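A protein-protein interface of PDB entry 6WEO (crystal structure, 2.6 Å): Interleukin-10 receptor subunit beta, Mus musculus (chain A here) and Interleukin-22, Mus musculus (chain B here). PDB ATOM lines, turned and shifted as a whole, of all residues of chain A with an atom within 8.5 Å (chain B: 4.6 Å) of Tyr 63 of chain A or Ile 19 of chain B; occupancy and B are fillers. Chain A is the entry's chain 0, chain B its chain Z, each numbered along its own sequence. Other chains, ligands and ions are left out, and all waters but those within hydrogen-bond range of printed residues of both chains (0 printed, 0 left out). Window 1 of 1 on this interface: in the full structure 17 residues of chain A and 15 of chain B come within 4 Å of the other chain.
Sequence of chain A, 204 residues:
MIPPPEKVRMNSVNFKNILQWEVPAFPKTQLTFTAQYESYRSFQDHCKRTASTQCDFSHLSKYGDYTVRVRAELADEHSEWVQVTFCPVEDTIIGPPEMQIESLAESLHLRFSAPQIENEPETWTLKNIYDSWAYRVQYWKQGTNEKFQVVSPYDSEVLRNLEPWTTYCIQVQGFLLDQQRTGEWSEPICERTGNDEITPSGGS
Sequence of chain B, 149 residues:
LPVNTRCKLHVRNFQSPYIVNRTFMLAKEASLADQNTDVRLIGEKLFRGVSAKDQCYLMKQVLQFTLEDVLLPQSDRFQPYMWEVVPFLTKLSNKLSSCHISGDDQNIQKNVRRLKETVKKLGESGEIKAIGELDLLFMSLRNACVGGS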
ATOM      1  N   PHE A  15      -2.417 -17.871 -24.487  1.00  0.00           N
ATOM      2  CA  PHE A  15      -2.216 -16.420 -24.535  1.00  0.00           C
ATOM      3  C   PHE A  15      -3.282 -15.713 -25.386  1.00  0.00           C
ATOM      4  O   PHE A  15      -3.060 -14.562 -25.834  1.00  0.00           O
ATOM      5  CB  PHE A  15      -0.808 -16.111 -25.019  1.00  0.00           C
ATOM      6  CG  PHE A  15       0.250 -16.519 -24.049  1.00  0.00           C
ATOM      7  CD1 PHE A  15       0.855 -17.764 -24.147  1.00  0.00           C
ATOM      8  CD2 PHE A  15       0.592 -15.698 -22.979  1.00  0.00           C
ATOM      9  CE1 PHE A  15       1.825 -18.170 -23.235  1.00  0.00           C
ATOM     10  CE2 PHE A  15       1.573 -16.087 -22.062  1.00  0.00           C
ATOM     11  CZ  PHE A  15       2.180 -17.330 -22.186  1.00  0.00           C
ATOM     12  N   GLU A  38      -5.208  -1.926 -16.499  1.00  0.00           N
ATOM     13  CA  GLU A  38      -4.348  -0.992 -15.774  1.00  0.00           C
ATOM     14  C   GLU A  38      -3.093  -0.649 -16.573  1.00  0.00           C
ATOM     15  O   GLU A  38      -2.437  -1.530 -17.126  1.00  0.00           O
ATOM     16  CB  GLU A  38      -3.994  -1.562 -14.394  1.00  0.00           C
ATOM     17  CG  GLU A  38      -3.081  -2.813 -14.362  1.00  0.00           C
ATOM     18  CD  GLU A  38      -1.594  -2.510 -14.430  1.00  0.00           C
ATOM     19  OE1 GLU A  38      -1.207  -1.371 -14.121  1.00  0.00           O
ATOM     20  OE2 GLU A  38      -0.807  -3.413 -14.797  1.00  0.00           O
ATOM     21  N   LEU A  60      -2.331  -7.760 -24.403  1.00  0.00           N
ATOM     22  CA  LEU A  60      -1.608  -7.528 -23.158  1.00  0.00           C
ATOM     23  C   LEU A  60      -0.272  -8.242 -23.185  1.00  0.00           C
ATOM     24  O   LEU A  60      -0.130  -9.307 -23.795  1.00  0.00           O
ATOM     25  CB  LEU A  60      -2.403  -8.044 -21.954  1.00  0.00           C
ATOM     26  CG  LEU A  60      -3.820  -7.516 -21.688  1.00  0.00           C
ATOM     27  CD1 LEU A  60      -4.378  -8.138 -20.401  1.00  0.00           C
ATOM     28  CD2 LEU A  60      -3.840  -6.010 -21.671  1.00  0.00           C
ATOM     29  N   SER A  61       0.717  -7.635 -22.525  1.00  0.00           N
ATOM     30  CA  SER A  61       2.056  -8.224 -22.442  1.00  0.00           C
ATOM     31  C   SER A  61       2.012  -9.544 -21.671  1.00  0.00           C
ATOM     32  O   SER A  61       1.235  -9.712 -20.729  1.00  0.00           O
ATOM     33  CB  SER A  61       3.054  -7.259 -21.767  1.00  0.00           C
ATOM     34  OG  SER A  61       2.897  -7.209 -20.350  1.00  0.00           O
ATOM     35  N   LYS A  62       2.872 -10.490 -22.065  1.00  0.00           N
ATOM     36  CA  LYS A  62       2.880 -11.765 -21.357  1.00  0.00           C
ATOM     37  C   LYS A  62       3.347 -11.576 -19.929  1.00  0.00           C
ATOM     38  O   LYS A  62       2.709 -12.042 -18.979  1.00  0.00           O
ATOM     39  CB  LYS A  62       3.827 -12.766 -22.000  1.00  0.00           C
ATOM     40  CG  LYS A  62       3.431 -13.408 -23.259  1.00  0.00           C
ATOM     41  CD  LYS A  62       3.768 -12.518 -24.410  1.00  0.00           C
ATOM     42  CE  LYS A  62       3.470 -13.292 -25.601  1.00  0.00           C
ATOM     43  NZ  LYS A  62       2.188 -13.968 -25.275  1.00  0.00           N
ATOM     44  N   TYR A  63       4.415 -10.822 -19.748  1.00  0.00           N
ATOM     45  CA  TYR A  63       5.009 -10.785 -18.436  1.00  0.00           C
ATOM     46  C   TYR A  63       4.408  -9.685 -17.573  1.00  0.00           C
ATOM     47  O   TYR A  63       4.827  -9.514 -16.427  1.00  0.00           O
ATOM     48  CB  TYR A  63       6.528 -10.660 -18.609  1.00  0.00           C
ATOM     49  CG  TYR A  63       7.255 -11.993 -18.891  1.00  0.00           C
ATOM     50  CD1 TYR A  63       7.146 -12.648 -20.129  1.00  0.00           C
ATOM     51  CD2 TYR A  63       8.120 -12.552 -17.944  1.00  0.00           C
ATOM     52  CE1 TYR A  63       7.857 -13.863 -20.384  1.00  0.00           C
ATOM     53  CE2 TYR A  63       8.835 -13.743 -18.195  1.00  0.00           C
ATOM     54  CZ  TYR A  63       8.691 -14.386 -19.406  1.00  0.00           C
ATOM     55  OH  TYR A  63       9.371 -15.555 -19.646  1.00  0.00           O
ATOM     56  N   GLY A  64       3.398  -8.976 -18.093  1.00  0.00           N
ATOM     57  CA  GLY A  64       2.762  -7.917 -17.341  1.00  0.00           C
ATOM     58  C   GLY A  64       1.767  -8.489 -16.345  1.00  0.00           C
ATOM     59  O   GLY A  64       1.007  -9.408 -16.650  1.00  0.00           O
ATOM     60  N   ASP A  65       1.764  -7.899 -15.142  1.00  0.00           N
ATOM     61  CA  ASP A  65       0.752  -8.164 -14.125  1.00  0.00           C
ATOM     62  C   ASP A  65      -0.384  -7.177 -14.360  1.00  0.00           C
ATOM     63  O   ASP A  65      -0.237  -5.981 -14.093  1.00  0.00           O
ATOM     64  CB  ASP A  65       1.296  -7.999 -12.700  1.00  0.00           C
ATOM     65  CG  ASP A  65       2.095  -9.209 -12.194  1.00  0.00           C
ATOM     66  OD1 ASP A  65       1.660 -10.357 -12.405  1.00  0.00           O
ATOM     67  OD2 ASP A  65       3.109  -9.009 -11.488  1.00  0.00           O
ATOM     68  N   TYR A  66      -1.516  -7.663 -14.851  1.00  0.00           N
ATOM     69  CA  TYR A  66      -2.612  -6.774 -15.172  1.00  0.00           C
ATOM     70  C   TYR A  66      -3.816  -7.091 -14.304  1.00  0.00           C
ATOM     71  O   TYR A  66      -4.087  -8.243 -13.990  1.00  0.00           O
ATOM     72  CB  TYR A  66      -3.032  -6.884 -16.622  1.00  0.00           C
ATOM     73  CG  TYR A  66      -2.016  -6.435 -17.647  1.00  0.00           C
ATOM     74  CD1 TYR A  66      -1.713  -5.087 -17.812  1.00  0.00           C
ATOM     75  CD2 TYR A  66      -1.425  -7.353 -18.515  1.00  0.00           C
ATOM     76  CE1 TYR A  66      -0.793  -4.677 -18.774  1.00  0.00           C
ATOM     77  CE2 TYR A  66      -0.530  -6.949 -19.475  1.00  0.00           C
ATOM     78  CZ  TYR A  66      -0.221  -5.615 -19.608  1.00  0.00           C
ATOM     79  OH  TYR A  66       0.667  -5.221 -20.580  1.00  0.00           O
ATOM     80  N   PHE A  86      -4.844 -10.707 -13.200  1.00  0.00           N
ATOM     81  CA  PHE A  86      -4.478 -11.528 -14.353  1.00  0.00           C
ATOM     82  C   PHE A  86      -3.064 -11.209 -14.817  1.00  0.00           C
ATOM     83  O   PHE A  86      -2.725 -10.046 -15.050  1.00  0.00           O
ATOM     84  CB  PHE A  86      -5.470 -11.302 -15.483  1.00  0.00           C
ATOM     85  CG  PHE A  86      -5.108 -11.978 -16.770  1.00  0.00           C
ATOM     86  CD1 PHE A  86      -5.090 -13.360 -16.868  1.00  0.00           C
ATOM     87  CD2 PHE A  86      -4.859 -11.222 -17.914  1.00  0.00           C
ATOM     88  CE1 PHE A  86      -4.792 -13.990 -18.083  1.00  0.00           C
ATOM     89  CE2 PHE A  86      -4.553 -11.839 -19.132  1.00  0.00           C
ATOM     90  CZ  PHE A  86      -4.520 -13.226 -19.222  1.00  0.00           C
ATOM     91  N   CYS A  87      -2.252 -12.253 -14.961  1.00  0.00           N
ATOM     92  CA  CYS A  87      -0.910 -12.174 -15.537  1.00  0.00           C
ATOM     93  C   CYS A  87      -0.830 -13.278 -16.574  1.00  0.00           C
ATOM     94  O   CYS A  87      -0.937 -14.463 -16.210  1.00  0.00           O
ATOM     95  CB  CYS A  87       0.191 -12.356 -14.486  1.00  0.00           C
ATOM     96  SG  CYS A  87       1.921 -12.421 -15.133  1.00  0.00           S
ATOM     97  N   PRO A  88      -0.649 -12.958 -17.849  1.00  0.00           N
ATOM     98  CA  PRO A  88      -0.804 -14.001 -18.883  1.00  0.00           C
ATOM     99  C   PRO A  88       0.146 -15.199 -18.748  1.00  0.00           C
ATOM    100  O   PRO A  88      -0.332 -16.343 -18.719  1.00  0.00           O
ATOM    101  CB  PRO A  88      -0.566 -13.224 -20.188  1.00  0.00           C
ATOM    102  CG  PRO A  88      -0.835 -11.816 -19.836  1.00  0.00           C
ATOM    103  CD  PRO A  88      -0.386 -11.635 -18.428  1.00  0.00           C
ATOM    104  N   VAL A  89       1.469 -14.983 -18.667  1.00  0.00           N
ATOM    105  CA  VAL A  89       2.401 -16.116 -18.732  1.00  0.00           C
ATOM    106  C   VAL A  89       2.258 -17.023 -17.503  1.00  0.00           C
ATOM    107  O   VAL A  89       2.547 -18.225 -17.574  1.00  0.00           O
ATOM    108  CB  VAL A  89       3.861 -15.642 -18.922  1.00  0.00           C
ATOM    109  CG1 VAL A  89       4.293 -14.664 -17.837  1.00  0.00           C
ATOM    110  CG2 VAL A  89       4.806 -16.797 -19.033  1.00  0.00           C
ATOM    111  N   GLU A  90       1.786 -16.486 -16.376  1.00  0.00           N
ATOM    112  CA  GLU A  90       1.586 -17.291 -15.177  1.00  0.00           C
ATOM    113  C   GLU A  90       0.201 -17.936 -15.103  1.00  0.00           C
ATOM    114  O   GLU A  90       0.065 -19.005 -14.501  1.00  0.00           O
ATOM    115  CB  GLU A  90       1.797 -16.428 -13.929  1.00  0.00           C
ATOM    116  CG  GLU A  90       3.206 -15.966 -13.717  1.00  0.00           C
ATOM    117  CD  GLU A  90       3.314 -14.971 -12.580  1.00  0.00           C
ATOM    118  OE1 GLU A  90       2.257 -14.575 -12.045  1.00  0.00           O
ATOM    119  OE2 GLU A  90       4.451 -14.595 -12.213  1.00  0.00           O
ATOM    120  N   ASN A 119      -0.203 -13.921 -29.529  1.00  0.00           N
ATOM    121  CA  ASN A 119       0.320 -12.588 -29.257  1.00  0.00           C
ATOM    122  C   ASN A 119       1.150 -12.070 -30.409  1.00  0.00           C
ATOM    123  O   ASN A 119       1.097 -10.881 -30.736  1.00  0.00           O
ATOM    124  CB  ASN A 119       1.169 -12.539 -27.987  1.00  0.00           C
ATOM    125  CG  ASN A 119       1.528 -11.099 -27.611  1.00  0.00           C
ATOM    126  OD1 ASN A 119       0.677 -10.262 -27.402  1.00  0.00           O
ATOM    127  ND2 ASN A 119       2.796 -10.803 -27.573  1.00  0.00           N
ATOM    128  N   TRP A 124       5.305 -17.993 -33.032  1.00  0.00           N
ATOM    129  CA  TRP A 124       5.816 -18.370 -31.727  1.00  0.00           C
ATOM    130  C   TRP A 124       4.949 -19.442 -31.087  1.00  0.00           C
ATOM    131  O   TRP A 124       3.721 -19.357 -31.124  1.00  0.00           O
ATOM    132  CB  TRP A 124       5.860 -17.144 -30.824  1.00  0.00           C
ATOM    133  CG  TRP A 124       6.848 -16.170 -31.290  1.00  0.00           C
ATOM    134  CD1 TRP A 124       6.606 -15.105 -32.088  1.00  0.00           C
ATOM    135  CD2 TRP A 124       8.239 -16.134 -30.978  1.00  0.00           C
ATOM    136  NE1 TRP A 124       7.767 -14.412 -32.317  1.00  0.00           N
ATOM    137  CE2 TRP A 124       8.784 -15.025 -31.640  1.00  0.00           C
ATOM    138  CE3 TRP A 124       9.070 -16.929 -30.213  1.00  0.00           C
ATOM    139  CZ2 TRP A 124      10.113 -14.700 -31.563  1.00  0.00           C
ATOM    140  CZ3 TRP A 124      10.381 -16.607 -30.132  1.00  0.00           C
ATOM    141  CH2 TRP A 124      10.900 -15.504 -30.803  1.00  0.00           C
ATOM    142  N   ASN A 128       8.428 -21.608 -27.030  1.00  0.00           N
ATOM    143  CA  ASN A 128       9.346 -20.491 -27.222  1.00  0.00           C
ATOM    144  C   ASN A 128       9.330 -19.487 -26.088  1.00  0.00           C
ATOM    145  O   ASN A 128      10.227 -18.639 -26.063  1.00  0.00           O
ATOM    146  CB  ASN A 128       9.040 -19.687 -28.478  1.00  0.00           C
ATOM    147  CG  ASN A 128       9.235 -20.464 -29.725  1.00  0.00           C
ATOM    148  OD1 ASN A 128       8.453 -20.342 -30.665  1.00  0.00           O
ATOM    149  ND2 ASN A 128      10.290 -21.263 -29.760  1.00  0.00           N
ATOM    150  N   ILE A 129       8.348 -19.543 -25.187  1.00  0.00           N
ATOM    151  CA  ILE A 129       8.218 -18.576 -24.097  1.00  0.00           C
ATOM    152  C   ILE A 129       8.680 -19.149 -22.762  1.00  0.00           C
ATOM    153  O   ILE A 129       9.362 -18.470 -21.991  1.00  0.00           O
ATOM    154  CB  ILE A 129       6.755 -18.101 -23.984  1.00  0.00           C
ATOM    155  CG1 ILE A 129       6.148 -17.778 -25.363  1.00  0.00           C
ATOM    156  CG2 ILE A 129       6.654 -16.969 -22.939  1.00  0.00           C
ATOM    157  CD1 ILE A 129       4.779 -18.328 -25.475  1.00  0.00           C
ATOM    158  N   TYR A 130       8.333 -20.397 -22.479  1.00  0.00           N
ATOM    159  CA  TYR A 130       8.669 -21.021 -21.212  1.00  0.00           C
ATOM    160  C   TYR A 130      10.005 -21.708 -21.391  1.00  0.00           C
ATOM    161  O   TYR A 130      10.206 -22.483 -22.328  1.00  0.00           O
ATOM    162  CB  TYR A 130       7.611 -22.045 -20.819  1.00  0.00           C
ATOM    163  CG  TYR A 130       6.225 -21.457 -20.646  1.00  0.00           C
ATOM    164  CD1 TYR A 130       5.930 -20.630 -19.566  1.00  0.00           C
ATOM    165  CD2 TYR A 130       5.212 -21.703 -21.595  1.00  0.00           C
ATOM    166  CE1 TYR A 130       4.653 -20.081 -19.402  1.00  0.00           C
ATOM    167  CE2 TYR A 130       3.943 -21.154 -21.442  1.00  0.00           C
ATOM    168  CZ  TYR A 130       3.671 -20.339 -20.336  1.00  0.00           C
ATOM    169  OH  TYR A 130       2.425 -19.772 -20.143  1.00  0.00           O
ATOM    170  N   ASP A 131      10.900 -21.437 -20.471  1.00  0.00           N
ATOM    171  CA  ASP A 131      12.265 -21.922 -20.448  1.00  0.00           C
ATOM    172  C   ASP A 131      12.380 -23.370 -20.004  1.00  0.00           C
ATOM    173  O   ASP A 131      13.452 -23.967 -20.159  1.00  0.00           O
ATOM    174  CB  ASP A 131      12.988 -20.998 -19.504  1.00  0.00           C
ATOM    175  CG  ASP A 131      12.153 -20.747 -18.267  1.00  0.00           C
ATOM    176  OD1 ASP A 131      11.935 -21.723 -17.520  1.00  0.00           O
ATOM    177  OD2 ASP A 131      11.635 -19.611 -18.094  1.00  0.00           O
ATOM    178  N   SER B  16      14.398 -17.910 -21.524  1.00  0.00           N
ATOM    179  CA  SER B  16      13.196 -17.870 -22.342  1.00  0.00           C
ATOM    180  C   SER B  16      13.583 -17.396 -23.729  1.00  0.00           C
ATOM    181  O   SER B  16      14.016 -16.247 -23.874  1.00  0.00           O
ATOM    182  CB  SER B  16      12.171 -16.929 -21.718  1.00  0.00           C
ATOM    183  OG  SER B  16      11.120 -16.612 -22.605  1.00  0.00           O
ATOM    184  N   PRO B  17      13.487 -18.231 -24.761  1.00  0.00           N
ATOM    185  CA  PRO B  17      13.889 -17.765 -26.097  1.00  0.00           C
ATOM    186  C   PRO B  17      13.128 -16.528 -26.525  1.00  0.00           C
ATOM    187  O   PRO B  17      13.669 -15.682 -27.240  1.00  0.00           O
ATOM    188  CB  PRO B  17      13.590 -18.977 -27.001  1.00  0.00           C
ATOM    189  CG  PRO B  17      13.600 -20.157 -26.090  1.00  0.00           C
ATOM    190  CD  PRO B  17      13.071 -19.649 -24.765  1.00  0.00           C
ATOM    191  N   TYR B  18      11.868 -16.419 -26.116  1.00  0.00           N
ATOM    192  CA  TYR B  18      11.046 -15.270 -26.481  1.00  0.00           C
ATOM    193  C   TYR B  18      11.581 -13.990 -25.871  1.00  0.00           C
ATOM    194  O   TYR B  18      11.811 -13.000 -26.575  1.00  0.00           O
ATOM    195  CB  TYR B  18       9.609 -15.509 -26.039  1.00  0.00           C
ATOM    196  CG  TYR B  18       8.674 -14.383 -26.344  1.00  0.00           C
ATOM    197  CD1 TYR B  18       8.136 -14.231 -27.613  1.00  0.00           C
ATOM    198  CD2 TYR B  18       8.278 -13.491 -25.348  1.00  0.00           C
ATOM    199  CE1 TYR B  18       7.259 -13.195 -27.890  1.00  0.00           C
ATOM    200  CE2 TYR B  18       7.397 -12.459 -25.610  1.00  0.00           C
ATOM    201  CZ  TYR B  18       6.895 -12.316 -26.874  1.00  0.00           C
ATOM    202  OH  TYR B  18       6.022 -11.289 -27.101  1.00  0.00           O
ATOM    203  N   ILE B  19      11.765 -13.984 -24.551  1.00  0.00           N
ATOM    204  CA  ILE B  19      12.174 -12.769 -23.866  1.00  0.00           C
ATOM    205  C   ILE B  19      13.570 -12.350 -24.313  1.00  0.00           C
ATOM    206  O   ILE B  19      13.851 -11.150 -24.428  1.00  0.00           O
ATOM    207  CB  ILE B  19      12.071 -12.977 -22.345  1.00  0.00           C
ATOM    208  CG1 ILE B  19      10.924 -12.156 -21.761  1.00  0.00           C
ATOM    209  CG2 ILE B  19      13.360 -12.505 -21.624  1.00  0.00           C
ATOM    210  CD1 ILE B  19       9.694 -12.170 -22.550  1.00  0.00           C
ATOM    211  N   VAL B  20      14.461 -13.318 -24.604  1.00  0.00           N
ATOM    212  CA  VAL B  20      15.822 -12.991 -25.039  1.00  0.00           C
ATOM    213  C   VAL B  20      15.804 -12.366 -26.428  1.00  0.00           C
ATOM    214  O   VAL B  20      16.510 -11.381 -26.694  1.00  0.00           O
ATOM    215  CB  VAL B  20      16.729 -14.244 -24.974  1.00  0.00           C
ATOM    216  CG1 VAL B  20      18.020 -14.066 -25.763  1.00  0.00           C
ATOM    217  CG2 VAL B  20      17.105 -14.506 -23.540  1.00  0.00           C
ATOM    218  N   ASN B  21      14.982 -12.913 -27.324  1.00  0.00           N
ATOM    219  CA  ASN B  21      14.845 -12.340 -28.656  1.00  0.00           C
ATOM    220  C   ASN B  21      14.303 -10.918 -28.587  1.00  0.00           C
ATOM    221  O   ASN B  21      14.879 -10.004 -29.185  1.00  0.00           O
ATOM    222  CB  ASN B  21      13.945 -13.249 -29.511  1.00  0.00           C
ATOM    223  CG  ASN B  21      13.728 -12.713 -30.903  1.00  0.00           C
ATOM    224  OD1 ASN B  21      12.819 -11.936 -31.132  1.00  0.00           O
ATOM    225  ND2 ASN B  21      14.549 -13.134 -31.841  1.00  0.00           N
ATOM    226  N   ARG B  22      13.272 -10.689 -27.773  1.00  0.00           N
ATOM    227  CA  ARG B  22      12.674  -9.361 -27.720  1.00  0.00           C
ATOM    228  C   ARG B  22      13.587  -8.351 -27.017  1.00  0.00           C
ATOM    229  O   ARG B  22      13.598  -7.158 -27.370  1.00  0.00           O
ATOM    230  CB  ARG B  22      11.286  -9.443 -27.088  1.00  0.00           C
ATOM    231  CG  ARG B  22      10.334 -10.242 -27.967  1.00  0.00           C
ATOM    232  CD  ARG B  22      10.089  -9.329 -29.138  1.00  0.00           C
ATOM    233  NE  ARG B  22       8.982  -9.648 -30.026  1.00  0.00           N
ATOM    234  CZ  ARG B  22       9.133 -10.107 -31.263  1.00  0.00           C
ATOM    235  NH1 ARG B  22      10.357 -10.293 -31.759  1.00  0.00           N
ATOM    236  NH2 ARG B  22       8.058 -10.352 -32.015  1.00  0.00           N
ATOM    237  N   THR B  23      14.299  -8.786 -25.979  1.00  0.00           N
ATOM    238  CA  THR B  23      15.260  -7.907 -25.327  1.00  0.00           C
ATOM    239  C   THR B  23      16.420  -7.555 -26.250  1.00  0.00           C
ATOM    240  O   THR B  23      16.893  -6.412 -26.252  1.00  0.00           O
ATOM    241  CB  THR B  23      15.746  -8.558 -24.034  1.00  0.00           C
ATOM    242  OG1 THR B  23      14.597  -8.905 -23.244  1.00  0.00           O
ATOM    243  CG2 THR B  23      16.684  -7.625 -23.253  1.00  0.00           C
ATOM    244  N   PRO B  87       7.645  -5.157 -19.124  1.00  0.00           N
ATOM    245  CA  PRO B  87       7.042  -6.005 -18.082  1.00  0.00           C
ATOM    246  C   PRO B  87       7.976  -7.105 -17.629  1.00  0.00           C
ATOM    247  O   PRO B  87       7.906  -7.541 -16.475  1.00  0.00           O
ATOM    248  CB  PRO B  87       5.808  -6.588 -18.772  1.00  0.00           C
ATOM    249  CG  PRO B  87       5.561  -5.705 -19.901  1.00  0.00           C
ATOM    250  CD  PRO B  87       6.896  -5.284 -20.382  1.00  0.00           C
ATOM    251  N   PHE B  88       8.841  -7.586 -18.522  1.00  0.00           N
ATOM    252  CA  PHE B  88       9.798  -8.603 -18.118  1.00  0.00           C
ATOM    253  C   PHE B  88      10.835  -8.014 -17.165  1.00  0.00           C
ATOM    254  O   PHE B  88      11.096  -8.581 -16.101  1.00  0.00           O
ATOM    255  CB  PHE B  88      10.482  -9.224 -19.343  1.00  0.00           C
ATOM    256  CG  PHE B  88      11.667 -10.063 -18.986  1.00  0.00           C
ATOM    257  CD1 PHE B  88      11.484 -11.318 -18.394  1.00  0.00           C
ATOM    258  CD2 PHE B  88      12.960  -9.595 -19.179  1.00  0.00           C
ATOM    259  CE1 PHE B  88      12.574 -12.092 -18.015  1.00  0.00           C
ATOM    260  CE2 PHE B  88      14.058 -10.378 -18.793  1.00  0.00           C
ATOM    261  CZ  PHE B  88      13.855 -11.624 -18.213  1.00  0.00           C
ATOM    262  N   LYS B  91       9.493  -7.475 -13.704  1.00  0.00           N
ATOM    263  CA  LYS B  91       9.416  -8.706 -12.932  1.00  0.00           C
ATOM    264  C   LYS B  91      10.755  -9.070 -12.337  1.00  0.00           C
ATOM    265  O   LYS B  91      10.793  -9.695 -11.272  1.00  0.00           O
ATOM    266  CB  LYS B  91       8.894  -9.863 -13.794  1.00  0.00           C
ATOM    267  CG  LYS B  91       7.458  -9.671 -14.200  1.00  0.00           C
ATOM    268  CD  LYS B  91       6.610  -9.608 -12.956  1.00  0.00           C
ATOM    269  CE  LYS B  91       5.164  -9.450 -13.281  1.00  0.00           C
ATOM    270  NZ  LYS B  91       4.534 -10.645 -13.902  1.00  0.00           N
ATOM    271  N   PHE B 138      20.861  -7.109 -19.449  1.00  0.00           N
ATOM    272  CA  PHE B 138      20.377  -8.488 -19.347  1.00  0.00           C
ATOM    273  C   PHE B 138      21.496  -9.436 -18.939  1.00  0.00           C
ATOM    274  O   PHE B 138      21.339 -10.237 -18.014  1.00  0.00           O
ATOM    275  CB  PHE B 138      19.793  -8.931 -20.691  1.00  0.00           C
ATOM    276  CG  PHE B 138      19.221 -10.330 -20.694  1.00  0.00           C
ATOM    277  CD1 PHE B 138      20.039 -11.448 -20.859  1.00  0.00           C
ATOM    278  CD2 PHE B 138      17.845 -10.520 -20.571  1.00  0.00           C
ATOM    279  CE1 PHE B 138      19.485 -12.717 -20.870  1.00  0.00           C
ATOM    280  CE2 PHE B 138      17.284 -11.792 -20.584  1.00  0.00           C
ATOM    281  CZ  PHE B 138      18.108 -12.891 -20.735  1.00  0.00           C
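The side-chain amino group of Lys 91 of chain B lies within hydrogen-bond range of the backbone carbonyl oxygen of Tyr 63 of chain A, at 2.8 Å.
The side-chain carboxylate of Asp 65 of chain A is in salt-bridge range of the side-chain amino group of Lys 91 of chain B, 3.2 Å away.
SG of Cys 87 of chain A is in hydrogen-bond range of NZ of Lys 91 of chain B, 3.4 Å away.
ND2 of Asn 119 of chain A lies within hydrogen-bond range of OH of Tyr 18 of chain B (3.3 Å).
The backbone carbonyl oxygen (O) of Asn 128 of chain A is in hydrogen-bond range of the backbone NH (N) of Tyr 18 of chain B, 2.8 Å away.
OG of Ser 16 of chain B sits at hydrogen-bond distance from O of Ile 129 of chain A, 2.6 Å away.
The side-chain carboxylate (OE2) of Glu 38 of chain A sits close to the backbone carbonyl oxygen (O) of Asp 65 of chain A, 2.7 Å away.
The backbone NH (N) of Gly 64 of chain A is in hydrogen-bond range of the side-chain hydroxyl (OG) of Ser 61 of chain A.
The side-chain hydroxyl of Ser 61 of chain A lies within hydrogen-bond range of the side-chain hydroxyl of Tyr 66 of chain A, at 3.0 Å.
The side-chain sulfur (SG) of Cys 87 of chain A is in hydrogen-bond range of the backbone carbonyl oxygen (O) of Gly 64 of chain A.
The side-chain sulfur (SG) of Cys 87 of chain A sits at hydrogen-bond distance from the side-chain carboxylate (OE1) of Glu 90 of chain A.
OG of Ser 16 of chain B is in hydrogen-bond range of N of Ile 19 of chain B, at 3.3 Å.
OG of Ser 61 of chain A touches CG of Pro 87 of chain B, at 3.1 Å.
CE of Lys 62 of chain A touches OH of Tyr 18 of chain B, 3.6 Å away.
Tyr 63 of chain A touches Ser 16 of chain B (OH to OG, 3.6 Å).
Ile 19 of chain B touches Tyr 63 of chain A (CD1 to CE1, 3.3 Å).
Tyr 63 of chain A touches Pro 87 of chain B (C to CB, 3.6 Å).
Tyr 63 of chain A touches Phe 88 of chain B (CE2 to CD1, 3.6 Å).
CD1 of Tyr 18 of chain B touches CE3 of Trp 124 of chain A, 3.9 Å away.
Asn 21 of chain B touches Trp 124 of chain A (OD1 to CZ2, 3.9 Å).
CA of Ile 129 of chain A touches CB of Tyr 18 of chain B, at 3.9 Å.
Ser 16 of chain B touches Asp 131 of chain A (N to CB, 3.95 Å).
Of chain B, only Ser 16 (3.6 Å), Ile 19 (3.3 Å), Pro 87 (3.6 Å), Phe 88 (3.6 Å) and Lys 91 (2.8 Å) come within 4 Å of Tyr 63 of chain A.
Of the printed residues of chain B, Ile 129 of chain A touches Ser 16 and Tyr 18.
Of the printed residues of chain B, Asp 65 of chain A touches Lys 91 (2.8 Å).
Printed residues of chain B within 4 Å of Gly 64 of chain A: Pro 87.
Printed residues of chain A within 4 Å of Pro 17 of chain B: Asn 128.
The nearest printed residue of chain B that does not touch Tyr 63 of chain A is Tyr 18 of chain B (5.0 Å).
Of the 20 printed residues of chain A, 11 touch a printed residue of chain B.
Hydrophobic or aromatic side chains of chain A that line the printed part of chain B: Tyr 63 and Trp 124.
Of the 12 printed residues of chain B, 8 touch a printed residue of chain A.
Hydrophobic or aromatic side chains of chain B within 4 Å of the printed part of chain A: Pro 17, Tyr 18, Ile 19, Pro 87 and Phe 88.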
